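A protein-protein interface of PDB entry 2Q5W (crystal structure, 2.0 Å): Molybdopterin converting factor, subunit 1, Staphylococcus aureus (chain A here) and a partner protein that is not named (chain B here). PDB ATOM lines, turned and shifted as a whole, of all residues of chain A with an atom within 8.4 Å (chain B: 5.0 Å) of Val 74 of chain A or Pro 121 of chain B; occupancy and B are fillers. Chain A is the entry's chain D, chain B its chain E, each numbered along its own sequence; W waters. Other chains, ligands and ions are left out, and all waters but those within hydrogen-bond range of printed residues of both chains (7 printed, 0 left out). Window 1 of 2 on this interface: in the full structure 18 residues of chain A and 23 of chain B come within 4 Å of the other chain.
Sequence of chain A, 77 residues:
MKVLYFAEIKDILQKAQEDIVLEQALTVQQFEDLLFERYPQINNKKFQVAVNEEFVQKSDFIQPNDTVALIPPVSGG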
ATOM      1  N   PHE A   6      11.417 -26.364   6.490  1.00  0.00           N
ATOM      2  CA  PHE A   6      11.265 -25.241   5.562  1.00  0.00           C
ATOM      3  C   PHE A   6      10.349 -24.192   6.154  1.00  0.00           C
ATOM      4  O   PHE A   6       9.468 -24.491   6.949  1.00  0.00           O
ATOM      5  CB  PHE A   6      10.716 -25.735   4.184  1.00  0.00           C
ATOM      6  CG  PHE A   6      11.663 -26.660   3.487  1.00  0.00           C
ATOM      7  CD1 PHE A   6      11.602 -28.027   3.702  1.00  0.00           C
ATOM      8  CD2 PHE A   6      12.708 -26.152   2.746  1.00  0.00           C
ATOM      9  CE1 PHE A   6      12.555 -28.894   3.132  1.00  0.00           C
ATOM     10  CE2 PHE A   6      13.630 -27.016   2.145  1.00  0.00           C
ATOM     11  CZ  PHE A   6      13.556 -28.386   2.372  1.00  0.00           C
ATOM     12  N   ALA A   7      10.607 -22.951   5.763  1.00  0.00           N
ATOM     13  CA  ALA A   7       9.682 -21.840   5.956  1.00  0.00           C
ATOM     14  C   ALA A   7       9.417 -21.606   7.423  1.00  0.00           C
ATOM     15  O   ALA A   7      10.365 -21.599   8.205  1.00  0.00           O
ATOM     16  CB  ALA A   7       8.408 -22.050   5.131  1.00  0.00           C
ATOM     17  N   LYS A  46       0.428 -26.489  10.202  1.00  0.00           N
ATOM     18  CA  LYS A  46      -0.087 -27.323   9.133  1.00  0.00           C
ATOM     19  C   LYS A  46       1.070 -27.676   8.217  1.00  0.00           C
ATOM     20  O   LYS A  46       1.891 -26.821   7.884  1.00  0.00           O
ATOM     21  CB  LYS A  46      -1.164 -26.553   8.386  1.00  0.00           C
ATOM     22  CG  LYS A  46      -1.894 -27.313   7.302  1.00  0.00           C
ATOM     23  CD  LYS A  46      -3.122 -26.538   6.851  1.00  0.00           C
ATOM     24  CE  LYS A  46      -3.964 -27.341   5.890  1.00  0.00           C
ATOM     25  NZ  LYS A  46      -5.358 -26.917   6.050  1.00  0.00           N
ATOM     26  N   PHE A  47       1.123 -28.926   7.776  1.00  0.00           N
ATOM     27  CA  PHE A  47       2.112 -29.308   6.806  1.00  0.00           C
ATOM     28  C   PHE A  47       1.781 -30.659   6.187  1.00  0.00           C
ATOM     29  O   PHE A  47       1.036 -31.442   6.758  1.00  0.00           O
ATOM     30  CB  PHE A  47       3.506 -29.326   7.456  1.00  0.00           C
ATOM     31  CG  PHE A  47       3.626 -30.259   8.627  1.00  0.00           C
ATOM     32  CD1 PHE A  47       3.912 -31.603   8.434  1.00  0.00           C
ATOM     33  CD2 PHE A  47       3.483 -29.792   9.927  1.00  0.00           C
ATOM     34  CE1 PHE A  47       4.026 -32.467   9.484  1.00  0.00           C
ATOM     35  CE2 PHE A  47       3.607 -30.655  10.984  1.00  0.00           C
ATOM     36  CZ  PHE A  47       3.874 -32.008  10.758  1.00  0.00           C
ATOM     37  N   GLN A  48       2.297 -30.896   4.978  1.00  0.00           N
ATOM     38  CA  GLN A  48       2.351 -32.231   4.398  1.00  0.00           C
ATOM     39  C   GLN A  48       3.753 -32.802   4.711  1.00  0.00           C
ATOM     40  O   GLN A  48       4.672 -32.076   5.059  1.00  0.00           O
ATOM     41  CB  GLN A  48       2.205 -32.140   2.886  1.00  0.00           C
ATOM     42  CG  GLN A  48       0.861 -31.649   2.439  1.00  0.00           C
ATOM     43  CD  GLN A  48       0.711 -31.675   0.936  1.00  0.00           C
ATOM     44  OE1 GLN A  48       0.413 -32.730   0.352  1.00  0.00           O
ATOM     45  NE2 GLN A  48       0.910 -30.512   0.293  1.00  0.00           N
ATOM     46  N   ALA A  50       6.814 -35.171   2.937  1.00  0.00           N
ATOM     47  CA  ALA A  50       7.386 -35.808   1.777  1.00  0.00           C
ATOM     48  C   ALA A  50       8.472 -36.753   2.258  1.00  0.00           C
ATOM     49  O   ALA A  50       9.224 -36.466   3.234  1.00  0.00           O
ATOM     50  CB  ALA A  50       7.962 -34.791   0.811  1.00  0.00           C
ATOM     51  N   GLU A  53      11.272 -37.077  -1.534  1.00  0.00           N
ATOM     52  CA  GLU A  53      10.817 -36.097  -2.505  1.00  0.00           C
ATOM     53  C   GLU A  53       9.490 -36.482  -3.124  1.00  0.00           C
ATOM     54  O   GLU A  53       9.167 -36.027  -4.209  1.00  0.00           O
ATOM     55  CB  GLU A  53      11.898 -35.811  -3.574  1.00  0.00           C
ATOM     56  CG  GLU A  53      13.197 -35.392  -2.936  1.00  0.00           C
ATOM     57  CD  GLU A  53      14.393 -35.444  -3.820  1.00  0.00           C
ATOM     58  OE1 GLU A  53      14.257 -35.708  -5.042  1.00  0.00           O
ATOM     59  OE2 GLU A  53      15.502 -35.199  -3.261  1.00  0.00           O
ATOM     60  N   PHE A  55       5.241 -36.717  -1.945  1.00  0.00           N
ATOM     61  CA  PHE A  55       4.260 -36.571  -0.891  1.00  0.00           C
ATOM     62  C   PHE A  55       3.788 -37.937  -0.413  1.00  0.00           C
ATOM     63  O   PHE A  55       3.509 -38.800  -1.226  1.00  0.00           O
ATOM     64  CB  PHE A  55       3.048 -35.773  -1.367  1.00  0.00           C
ATOM     65  CG  PHE A  55       3.340 -34.314  -1.557  1.00  0.00           C
ATOM     66  CD1 PHE A  55       3.175 -33.717  -2.788  1.00  0.00           C
ATOM     67  CD2 PHE A  55       3.812 -33.553  -0.489  1.00  0.00           C
ATOM     68  CE1 PHE A  55       3.446 -32.365  -2.959  1.00  0.00           C
ATOM     69  CE2 PHE A  55       4.113 -32.219  -0.662  1.00  0.00           C
ATOM     70  CZ  PHE A  55       3.912 -31.611  -1.881  1.00  0.00           C
ATOM     71  N   ALA A  69      10.770 -34.618   4.660  1.00  0.00           N
ATOM     72  CA  ALA A  69      10.663 -33.136   4.660  1.00  0.00           C
ATOM     73  C   ALA A  69       9.269 -32.687   5.096  1.00  0.00           C
ATOM     74  O   ALA A  69       8.283 -33.298   4.718  1.00  0.00           O
ATOM     75  CB  ALA A  69      10.992 -32.554   3.255  1.00  0.00           C
ATOM     76  N   LEU A  70       9.207 -31.657   5.935  1.00  0.00           N
ATOM     77  CA  LEU A  70       7.945 -31.029   6.314  1.00  0.00           C
ATOM     78  C   LEU A  70       7.683 -29.860   5.337  1.00  0.00           C
ATOM     79  O   LEU A  70       8.500 -28.962   5.208  1.00  0.00           O
ATOM     80  CB  LEU A  70       7.986 -30.559   7.757  1.00  0.00           C
ATOM     81  CG  LEU A  70       8.261 -31.616   8.842  1.00  0.00           C
ATOM     82  CD1 LEU A  70       7.889 -30.995  10.161  1.00  0.00           C
ATOM     83  CD2 LEU A  70       7.454 -32.871   8.607  1.00  0.00           C
ATOM     84  N   ILE A  71       6.533 -29.923   4.666  1.00  0.00           N
ATOM     85  CA  ILE A  71       6.140 -29.016   3.599  1.00  0.00           C
ATOM     86  C   ILE A  71       4.924 -28.220   4.066  1.00  0.00           C
ATOM     87  O   ILE A  71       3.779 -28.675   3.953  1.00  0.00           O
ATOM     88  CB  ILE A  71       5.771 -29.827   2.335  1.00  0.00           C
ATOM     89  CG1 ILE A  71       6.916 -30.769   1.917  1.00  0.00           C
ATOM     90  CG2 ILE A  71       5.322 -28.936   1.201  1.00  0.00           C
ATOM     91  CD1 ILE A  71       8.231 -30.141   1.752  1.00  0.00           C
ATOM     92  N   PRO A  72       5.154 -27.011   4.574  1.00  0.00           N
ATOM     93  CA  PRO A  72       4.022 -26.160   4.928  1.00  0.00           C
ATOM     94  C   PRO A  72       3.239 -25.721   3.705  1.00  0.00           C
ATOM     95  O   PRO A  72       3.652 -26.019   2.567  1.00  0.00           O
ATOM     96  CB  PRO A  72       4.670 -24.965   5.639  1.00  0.00           C
ATOM     97  CG  PRO A  72       6.040 -25.409   5.992  1.00  0.00           C
ATOM     98  CD  PRO A  72       6.427 -26.405   4.927  1.00  0.00           C
ATOM     99  N   PRO A  73       2.097 -25.067   3.918  1.00  0.00           N
ATOM    100  CA  PRO A  73       1.255 -24.679   2.787  1.00  0.00           C
ATOM    101  C   PRO A  73       2.065 -23.815   1.812  1.00  0.00           C
ATOM    102  O   PRO A  73       2.726 -22.871   2.212  1.00  0.00           O
ATOM    103  CB  PRO A  73       0.110 -23.904   3.466  1.00  0.00           C
ATOM    104  CG  PRO A  73       0.031 -24.560   4.884  1.00  0.00           C
ATOM    105  CD  PRO A  73       1.479 -24.689   5.210  1.00  0.00           C
ATOM    106  N   VAL A  74       2.058 -24.183   0.552  1.00  0.00           N
ATOM    107  CA  VAL A  74       2.989 -23.590  -0.405  1.00  0.00           C
ATOM    108  C   VAL A  74       2.510 -22.223  -0.869  1.00  0.00           C
ATOM    109  O   VAL A  74       1.325 -21.944  -0.840  1.00  0.00           O
ATOM    110  CB  VAL A  74       3.202 -24.540  -1.588  1.00  0.00           C
ATOM    111  CG1 VAL A  74       3.736 -25.889  -1.035  1.00  0.00           C
ATOM    112  CG2 VAL A  74       1.941 -24.722  -2.367  1.00  0.00           C
ATOM    113  N   SER A  75       3.437 -21.358  -1.256  1.00  0.00           N
ATOM    114  CA  SER A  75       3.128 -19.957  -1.600  1.00  0.00           C
ATOM    115  C   SER A  75       4.094 -19.449  -2.701  1.00  0.00           C
ATOM    116  O   SER A  75       4.458 -18.259  -2.750  1.00  0.00           O
ATOM    117  CB  SER A  75       3.197 -19.088  -0.333  1.00  0.00           C
ATOM    118  OG  SER A  75       4.481 -19.140   0.286  1.00  0.00           O
ATOM    119  N   GLY A  76       4.481 -20.356  -3.608  1.00  0.00           N
ATOM    120  CA  GLY A  76       5.228 -19.963  -4.776  1.00  0.00           C
ATOM    121  C   GLY A  76       4.371 -19.355  -5.863  1.00  0.00           C
ATOM    122  O   GLY A  76       3.134 -19.367  -5.782  1.00  0.00           O
ATOM    123  N   GLY A  77       5.034 -18.822  -6.890  1.00  0.00           N
ATOM    124  CA  GLY A  77       4.371 -18.415  -8.099  1.00  0.00           C
ATOM    125  C   GLY A  77       4.004 -16.951  -8.102  1.00  0.00           C
ATOM    126  O   GLY A  77       4.228 -16.245  -7.111  1.00  0.00           O
ATOM    127  OXT GLY A  77       3.490 -16.448  -9.123  1.00  0.00           O
ATOM    128  N   GLU B  51      12.028 -19.463  -0.441  1.00  0.00           N
ATOM    129  CA  GLU B  51      12.676 -20.720  -0.140  1.00  0.00           C
ATOM    130  C   GLU B  51      12.028 -21.795  -1.012  1.00  0.00           C
ATOM    131  O   GLU B  51      10.860 -21.683  -1.405  1.00  0.00           O
ATOM    132  CB  GLU B  51      12.414 -21.137   1.310  1.00  0.00           C
ATOM    133  CG  GLU B  51      13.357 -20.602   2.295  1.00  0.00           C
ATOM    134  CD  GLU B  51      13.193 -21.197   3.698  1.00  0.00           C
ATOM    135  OE1 GLU B  51      12.556 -22.275   3.898  1.00  0.00           O
ATOM    136  OE2 GLU B  51      13.721 -20.527   4.594  1.00  0.00           O
ATOM    137  N   ALA B  52      12.771 -22.878  -1.239  1.00  0.00           N
ATOM    138  CA  ALA B  52      12.213 -24.063  -1.905  1.00  0.00           C
ATOM    139  C   ALA B  52      12.896 -25.313  -1.388  1.00  0.00           C
ATOM    140  O   ALA B  52      14.054 -25.273  -0.972  1.00  0.00           O
ATOM    141  CB  ALA B  52      12.376 -23.926  -3.405  1.00  0.00           C
ATOM    142  N   TYR B  53      12.167 -26.419  -1.402  1.00  0.00           N
ATOM    143  CA  TYR B  53      12.750 -27.744  -1.265  1.00  0.00           C
ATOM    144  C   TYR B  53      13.140 -28.083  -2.674  1.00  0.00           C
ATOM    145  O   TYR B  53      12.338 -28.621  -3.456  1.00  0.00           O
ATOM    146  CB  TYR B  53      11.719 -28.704  -0.737  1.00  0.00           C
ATOM    147  CG  TYR B  53      12.175 -30.113  -0.515  1.00  0.00           C
ATOM    148  CD1 TYR B  53      13.544 -30.458  -0.488  1.00  0.00           C
ATOM    149  CD2 TYR B  53      11.235 -31.125  -0.380  1.00  0.00           C
ATOM    150  CE1 TYR B  53      13.958 -31.740  -0.259  1.00  0.00           C
ATOM    151  CE2 TYR B  53      11.635 -32.433  -0.168  1.00  0.00           C
ATOM    152  CZ  TYR B  53      13.025 -32.736  -0.102  1.00  0.00           C
ATOM    153  OH  TYR B  53      13.420 -34.054   0.142  1.00  0.00           O
ATOM    154  N   MET B  56      12.677 -31.507  -4.861  1.00  0.00           N
ATOM    155  CA  MET B  56      11.253 -31.803  -5.032  1.00  0.00           C
ATOM    156  C   MET B  56      10.534 -30.745  -5.887  1.00  0.00           C
ATOM    157  O   MET B  56       9.687 -31.089  -6.746  1.00  0.00           O
ATOM    158  CB  MET B  56      10.585 -31.944  -3.678  1.00  0.00           C
ATOM    159  CG  MET B  56       9.234 -32.534  -3.741  1.00  0.00           C
ATOM    160  SD  MET B  56       8.502 -32.863  -2.164  1.00  0.00           S
ATOM    161  CE  MET B  56       6.962 -33.559  -2.801  1.00  0.00           C
ATOM    162  N   ALA B  57      10.872 -29.467  -5.685  1.00  0.00           N
ATOM    163  CA  ALA B  57      10.333 -28.387  -6.494  1.00  0.00           C
ATOM    164  C   ALA B  57      10.643 -28.570  -7.981  1.00  0.00           C
ATOM    165  O   ALA B  57       9.753 -28.416  -8.802  1.00  0.00           O
ATOM    166  CB  ALA B  57      10.844 -27.056  -6.013  1.00  0.00           C
ATOM    167  N   LYS B  60       8.487 -31.349  -9.286  1.00  0.00           N
ATOM    168  CA  LYS B  60       7.088 -30.935  -9.430  1.00  0.00           C
ATOM    169  C   LYS B  60       6.895 -29.979 -10.643  1.00  0.00           C
ATOM    170  O   LYS B  60       5.875 -30.005 -11.306  1.00  0.00           O
ATOM    171  CB  LYS B  60       6.570 -30.317  -8.129  1.00  0.00           C
ATOM    172  CG  LYS B  60       6.390 -31.350  -7.011  1.00  0.00           C
ATOM    173  CD  LYS B  60       5.155 -32.190  -7.276  1.00  0.00           C
ATOM    174  CE  LYS B  60       5.085 -33.394  -6.380  1.00  0.00           C
ATOM    175  NZ  LYS B  60       3.939 -34.297  -6.756  1.00  0.00           N
ATOM    176  N   ILE B 116       1.709 -24.390 -10.365  1.00  0.00           N
ATOM    177  CA  ILE B 116       2.826 -24.018  -9.531  1.00  0.00           C
ATOM    178  C   ILE B 116       2.316 -23.568  -8.156  1.00  0.00           C
ATOM    179  O   ILE B 116       2.858 -23.972  -7.133  1.00  0.00           O
ATOM    180  CB  ILE B 116       3.628 -22.897 -10.169  1.00  0.00           C
ATOM    181  CG1 ILE B 116       4.366 -23.437 -11.397  1.00  0.00           C
ATOM    182  CG2 ILE B 116       4.643 -22.281  -9.175  1.00  0.00           C
ATOM    183  CD1 ILE B 116       5.094 -22.368 -12.232  1.00  0.00           C
ATOM    184  N   LYS B 117       1.247 -22.770  -8.140  1.00  0.00           N
ATOM    185  CA  LYS B 117       0.710 -22.260  -6.897  1.00  0.00           C
ATOM    186  C   LYS B 117       0.060 -23.354  -6.072  1.00  0.00           C
ATOM    187  O   LYS B 117      -0.103 -23.214  -4.843  1.00  0.00           O
ATOM    188  CB  LYS B 117      -0.291 -21.134  -7.187  1.00  0.00           C
ATOM    189  CG  LYS B 117       0.372 -19.918  -7.835  1.00  0.00           C
ATOM    190  CD  LYS B 117      -0.605 -18.727  -8.027  1.00  0.00           C
ATOM    191  CE  LYS B 117       0.212 -17.431  -8.313  1.00  0.00           C
ATOM    192  NZ  LYS B 117      -0.047 -16.245  -7.395  1.00  0.00           N
ATOM    193  N   GLU B 118      -0.355 -24.419  -6.742  1.00  0.00           N
ATOM    194  CA  GLU B 118      -1.043 -25.510  -6.097  1.00  0.00           C
ATOM    195  C   GLU B 118      -0.065 -26.494  -5.452  1.00  0.00           C
ATOM    196  O   GLU B 118      -0.258 -26.883  -4.323  1.00  0.00           O
ATOM    197  CB  GLU B 118      -1.957 -26.243  -7.095  1.00  0.00           C
ATOM    198  CG  GLU B 118      -3.265 -25.491  -7.398  1.00  0.00           C
ATOM    199  CD  GLU B 118      -4.114 -26.047  -8.582  1.00  0.00           C
ATOM    200  OE1 GLU B 118      -3.717 -27.007  -9.276  1.00  0.00           O
ATOM    201  OE2 GLU B 118      -5.220 -25.491  -8.812  1.00  0.00           O
ATOM    202  N   ILE B 119       0.956 -26.932  -6.170  1.00  0.00           N
ATOM    203  CA  ILE B 119       1.650 -28.156  -5.777  1.00  0.00           C
ATOM    204  C   ILE B 119       3.152 -28.050  -5.509  1.00  0.00           C
ATOM    205  O   ILE B 119       3.739 -29.006  -5.027  1.00  0.00           O
ATOM    206  CB  ILE B 119       1.475 -29.278  -6.827  1.00  0.00           C
ATOM    207  CG1 ILE B 119       2.267 -28.982  -8.106  1.00  0.00           C
ATOM    208  CG2 ILE B 119      -0.020 -29.548  -7.062  1.00  0.00           C
ATOM    209  CD1 ILE B 119       2.306 -30.115  -9.107  1.00  0.00           C
ATOM    210  N   VAL B 120       3.786 -26.952  -5.896  1.00  0.00           N
ATOM    211  CA  VAL B 120       5.258 -26.938  -5.921  1.00  0.00           C
ATOM    212  C   VAL B 120       5.771 -26.424  -4.576  1.00  0.00           C
ATOM    213  O   VAL B 120       5.280 -25.389  -4.077  1.00  0.00           O
ATOM    214  CB  VAL B 120       5.774 -26.044  -7.038  1.00  0.00           C
ATOM    215  CG1 VAL B 120       7.294 -26.079  -7.094  1.00  0.00           C
ATOM    216  CG2 VAL B 120       5.227 -26.519  -8.379  1.00  0.00           C
ATOM    217  N   PRO B 121       6.653 -27.197  -3.908  1.00  0.00           N
ATOM    218  CA  PRO B 121       7.152 -26.752  -2.584  1.00  0.00           C
ATOM    219  C   PRO B 121       8.121 -25.573  -2.634  1.00  0.00           C
ATOM    220  O   PRO B 121       9.332 -25.752  -2.621  1.00  0.00           O
ATOM    221  CB  PRO B 121       7.762 -28.024  -1.995  1.00  0.00           C
ATOM    222  CG  PRO B 121       8.136 -28.835  -3.187  1.00  0.00           C
ATOM    223  CD  PRO B 121       7.091 -28.560  -4.231  1.00  0.00           C
ATOM    224  N   ILE B 122       7.533 -24.375  -2.664  1.00  0.00           N
ATOM    225  CA  ILE B 122       8.209 -23.090  -2.680  1.00  0.00           C
ATOM    226  C   ILE B 122       7.401 -22.216  -1.743  1.00  0.00           C
ATOM    227  O   ILE B 122       6.154 -22.308  -1.711  1.00  0.00           O
ATOM    228  CB  ILE B 122       8.193 -22.440  -4.078  1.00  0.00           C
ATOM    229  CG1 ILE B 122       8.967 -23.301  -5.076  1.00  0.00           C
ATOM    230  CG2 ILE B 122       8.784 -21.014  -4.065  1.00  0.00           C
ATOM    231  CD1 ILE B 122       8.657 -22.980  -6.524  1.00  0.00           C
ATOM    232  N   TRP B 123       8.092 -21.392  -0.972  1.00  0.00           N
ATOM    233  CA  TRP B 123       7.426 -20.535   0.005  1.00  0.00           C
ATOM    234  C   TRP B 123       7.935 -19.100  -0.081  1.00  0.00           C
ATOM    235  O   TRP B 123       9.113 -18.878  -0.326  1.00  0.00           O
ATOM    236  CB  TRP B 123       7.588 -21.082   1.431  1.00  0.00           C
ATOM    237  CG  TRP B 123       7.179 -22.463   1.583  1.00  0.00           C
ATOM    238  CD1 TRP B 123       5.947 -22.934   1.890  1.00  0.00           C
ATOM    239  CD2 TRP B 123       8.013 -23.600   1.379  1.00  0.00           C
ATOM    240  NE1 TRP B 123       5.971 -24.315   1.927  1.00  0.00           N
ATOM    241  CE2 TRP B 123       7.225 -24.738   1.586  1.00  0.00           C
ATOM    242  CE3 TRP B 123       9.348 -23.756   1.044  1.00  0.00           C
ATOM    243  CZ2 TRP B 123       7.733 -26.034   1.466  1.00  0.00           C
ATOM    244  CZ3 TRP B 123       9.850 -25.056   0.889  1.00  0.00           C
ATOM    245  CH2 TRP B 123       9.039 -26.165   1.103  1.00  0.00           C
ATOM    246  N   GLY B 136       0.940 -18.130   3.093  1.00  0.00           N
ATOM    247  CA  GLY B 136       0.372 -19.470   2.889  1.00  0.00           C
ATOM    248  C   GLY B 136      -0.430 -19.591   1.611  1.00  0.00           C
ATOM    249  O   GLY B 136      -0.267 -18.786   0.685  1.00  0.00           O
ATOM    250  N   HIS B 137      -1.263 -20.638   1.584  1.00  0.00           N
ATOM    251  CA  HIS B 137      -2.264 -20.966   0.529  1.00  0.00           C
ATOM    252  C   HIS B 137      -2.209 -22.478   0.267  1.00  0.00           C
ATOM    253  O   HIS B 137      -1.318 -22.963  -0.446  1.00  0.00           O
ATOM    254  CB  HIS B 137      -2.068 -20.192  -0.786  1.00  0.00           C
ATOM    255  CG  HIS B 137      -3.257 -19.390  -1.201  1.00  0.00           C
ATOM    256  ND1 HIS B 137      -3.981 -18.622  -0.312  1.00  0.00           N
ATOM    257  CD2 HIS B 137      -3.819 -19.187  -2.421  1.00  0.00           C
ATOM    258  CE1 HIS B 137      -4.964 -18.010  -0.959  1.00  0.00           C
ATOM    259  NE2 HIS B 137      -4.892 -18.339  -2.240  1.00  0.00           N
HETATM  260  O   HOH W   1       4.621 -36.512  -4.861  1.00  0.00           O
HETATM  261  O   HOH W   2       0.255 -21.127  -3.356  1.00  0.00           O
HETATM  262  O   HOH W   3       0.401 -28.197  -2.106  1.00  0.00           O
HETATM  263  O   HOH W   4      12.884 -20.513   7.284  1.00  0.00           O
HETATM  264  O   HOH W   5      11.591 -35.854   1.001  1.00  0.00           O
HETATM  265  O   HOH W   6      15.784 -34.499  -0.786  1.00  0.00           O
HETATM  266  O   HOH W   7       4.064 -23.042  -4.831  1.00  0.00           O
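Hydrophobic or aromatic side chains of chain B within 4 Å of the printed part of chain A: Tyr 53, Met 56, Ile 122, Trp 123 and His 137. Of the 17 printed residues of chain A, 13 touch a printed residue of chain B. Among the printed residues, 31 pairs touch across the chains. Among the printed residues, no Asp or Glu carboxylate lies within 4 Å of a Lys or Arg side-chain nitrogen of the other chain.
O of Ile 71 of chain A is in hydrogen-bond range of N of Gln 48 of chain A (2.9 Å). The backbone NH (N) of Trp 123 of chain B is in hydrogen-bond range of the backbone carbonyl oxygen (O) of Glu 51 of chain B (2.8 Å). O of Pro 121 of chain B sits at hydrogen-bond distance from N of Tyr 53 of chain B, 3.2 Å away. The backbone carbonyl oxygen (O) of Ala 50 of chain A lies within hydrogen-bond range of the backbone NH (N) of Ala 69 of chain A (2.8 Å).
Among the printed residues, merely in contact across the chains: Phe 6 of chain A with Glu 51 of chain B (3.6 Å), Phe 6 of chain A with Ala 52 of chain B (3.6 Å), Phe 6 of chain A with Tyr 53 of chain B (3.5 Å), Phe 6 of chain A with Trp 123 of chain B (3.5 Å), Ala 7 of chain A with Trp 123 of chain B (3.8 Å), Ala 50 of chain A with Met 56 of chain B (3.6 Å), Glu 53 of chain A with Tyr 53 of chain B (3.4 Å), Glu 53 of chain A with Met 56 of chain B (3.5 Å), Phe 55 of chain A with Met 56 of chain B (3.7 Å), Phe 55 of chain A with Lys 60 of chain B (3.9 Å), Phe 55 of chain A with Ile 119 of chain B (3.96 Å), Ala 69 of chain A with Tyr 53 of chain B (3.5 Å), Ile 71 of chain A with Tyr 53 of chain B (3.8 Å), Ile 71 of chain A with Trp 123 of chain B (3.8 Å), Pro 73 of chain A with Trp 123 of chain B (3.2 Å), Val 74 of chain A with Lys 117 of chain B (3.5 Å), Val 74 of chain A with Glu 118 of chain B (3.7 Å), Val 74 of chain A with Val 120 of chain B (3.4 Å), Val 74 of chain A with Pro 121 of chain B (3.8 Å), Val 74 of chain A with Ile 122 of chain B (3.7 Å), Val 74 of chain A with Trp 123 of chain B (3.8 Å), Val 74 of chain A with Gly 136 of chain B (3.8 Å), Ser 75 of chain A with Trp 123 of chain B (3.3 Å), Ser 75 of chain A with Gly 136 of chain B (3.6 Å) and Gly 76 of chain A with Lys 117 of chain B (3.5 Å).
Of the printed residues of chain B, Phe 6 of chain A touches Glu 51, Ala 52, Tyr 53 and Trp 123. Lys 46 of chain A touches none of the printed residues of chain B. Gln 48 of chain A touches none of the printed residues of chain B. Printed residues of chain A within 4 Å of Ala 52 of chain B: Phe 6. Of the printed residues of chain A, Tyr 53 of chain B touches Phe 6 (3.5 Å), Glu 53 (3.4 Å), Ala 69 (3.5 Å) and Ile 71 (3.8 Å). Of chain A, only Val 74 (3.8 Å) comes within 4 Å of Pro 121 of chain B. Printed residues of chain A within 4 Å of Gly 136 of chain B: Val 74 (3.8 Å) and Ser 75 (3.6 Å). The nearest residue of chain A that does not touch Pro 121 of chain B is Ile 71 of chain A (4.1 Å). The nearest printed residue of chain B that does not touch Gly 76 of chain A is Ile 116 of chain B (4.4 Å).
O of Val 74 of chain A lies close to O of His 137 of chain B, 2.9 Å away. NZ of Lys 117 of chain B is in salt-bridge range of OXT of Gly 77 of chain A. The backbone carbonyl oxygen of Ile 122 of chain B sits at hydrogen-bond distance from the backbone NH of Ser 75 of chain A (2.9 Å). The indole nitrogen (NE1) of Trp 123 of chain B is in hydrogen-bond range of the backbone carbonyl oxygen (O) of Pro 72 of chain A (2.9 Å). OE1 of Glu 51 of chain B is in hydrogen-bond range of N of Ala 7 of chain A (2.8 Å). The backbone NH (N) of Gly 76 of chain A sits at hydrogen-bond distance from the backbone carbonyl oxygen (O) of Ile 122 of chain B, at 3.2 Å.
Water W6 lies within hydrogen-bond range of OH of Tyr 53 of chain B (2.6 Å) and OE2 of Glu 53 of chain A (2.6 Å). Water W2 lies within hydrogen-bond range of O of Lys 117 of chain B (2.6 Å) and O of Val 74 of chain A (2.9 Å). Water W3 bridges O of Glu 118 of chain B and NE2 of Gln 48 of chain A. Water W5 lies within hydrogen-bond range of the side-chain hydroxyl (OH) of Tyr 53 of chain B (2.7 Å), the backbone NH (N) of Glu 53 of chain A (2.8 Å) and the backbone carbonyl oxygen (O) of Ala 50 of chain A (3.3 Å). Water W4 lies within hydrogen-bond range of OE2 of Glu 51 of chain B (2.8 Å) and O of Ala 7 of chain A (2.9 Å). Water W1 bridges the backbone NH of Phe 55 of chain A (3.0 Å) and the side-chain amino group of Lys 60 of chain B (3.0 Å).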
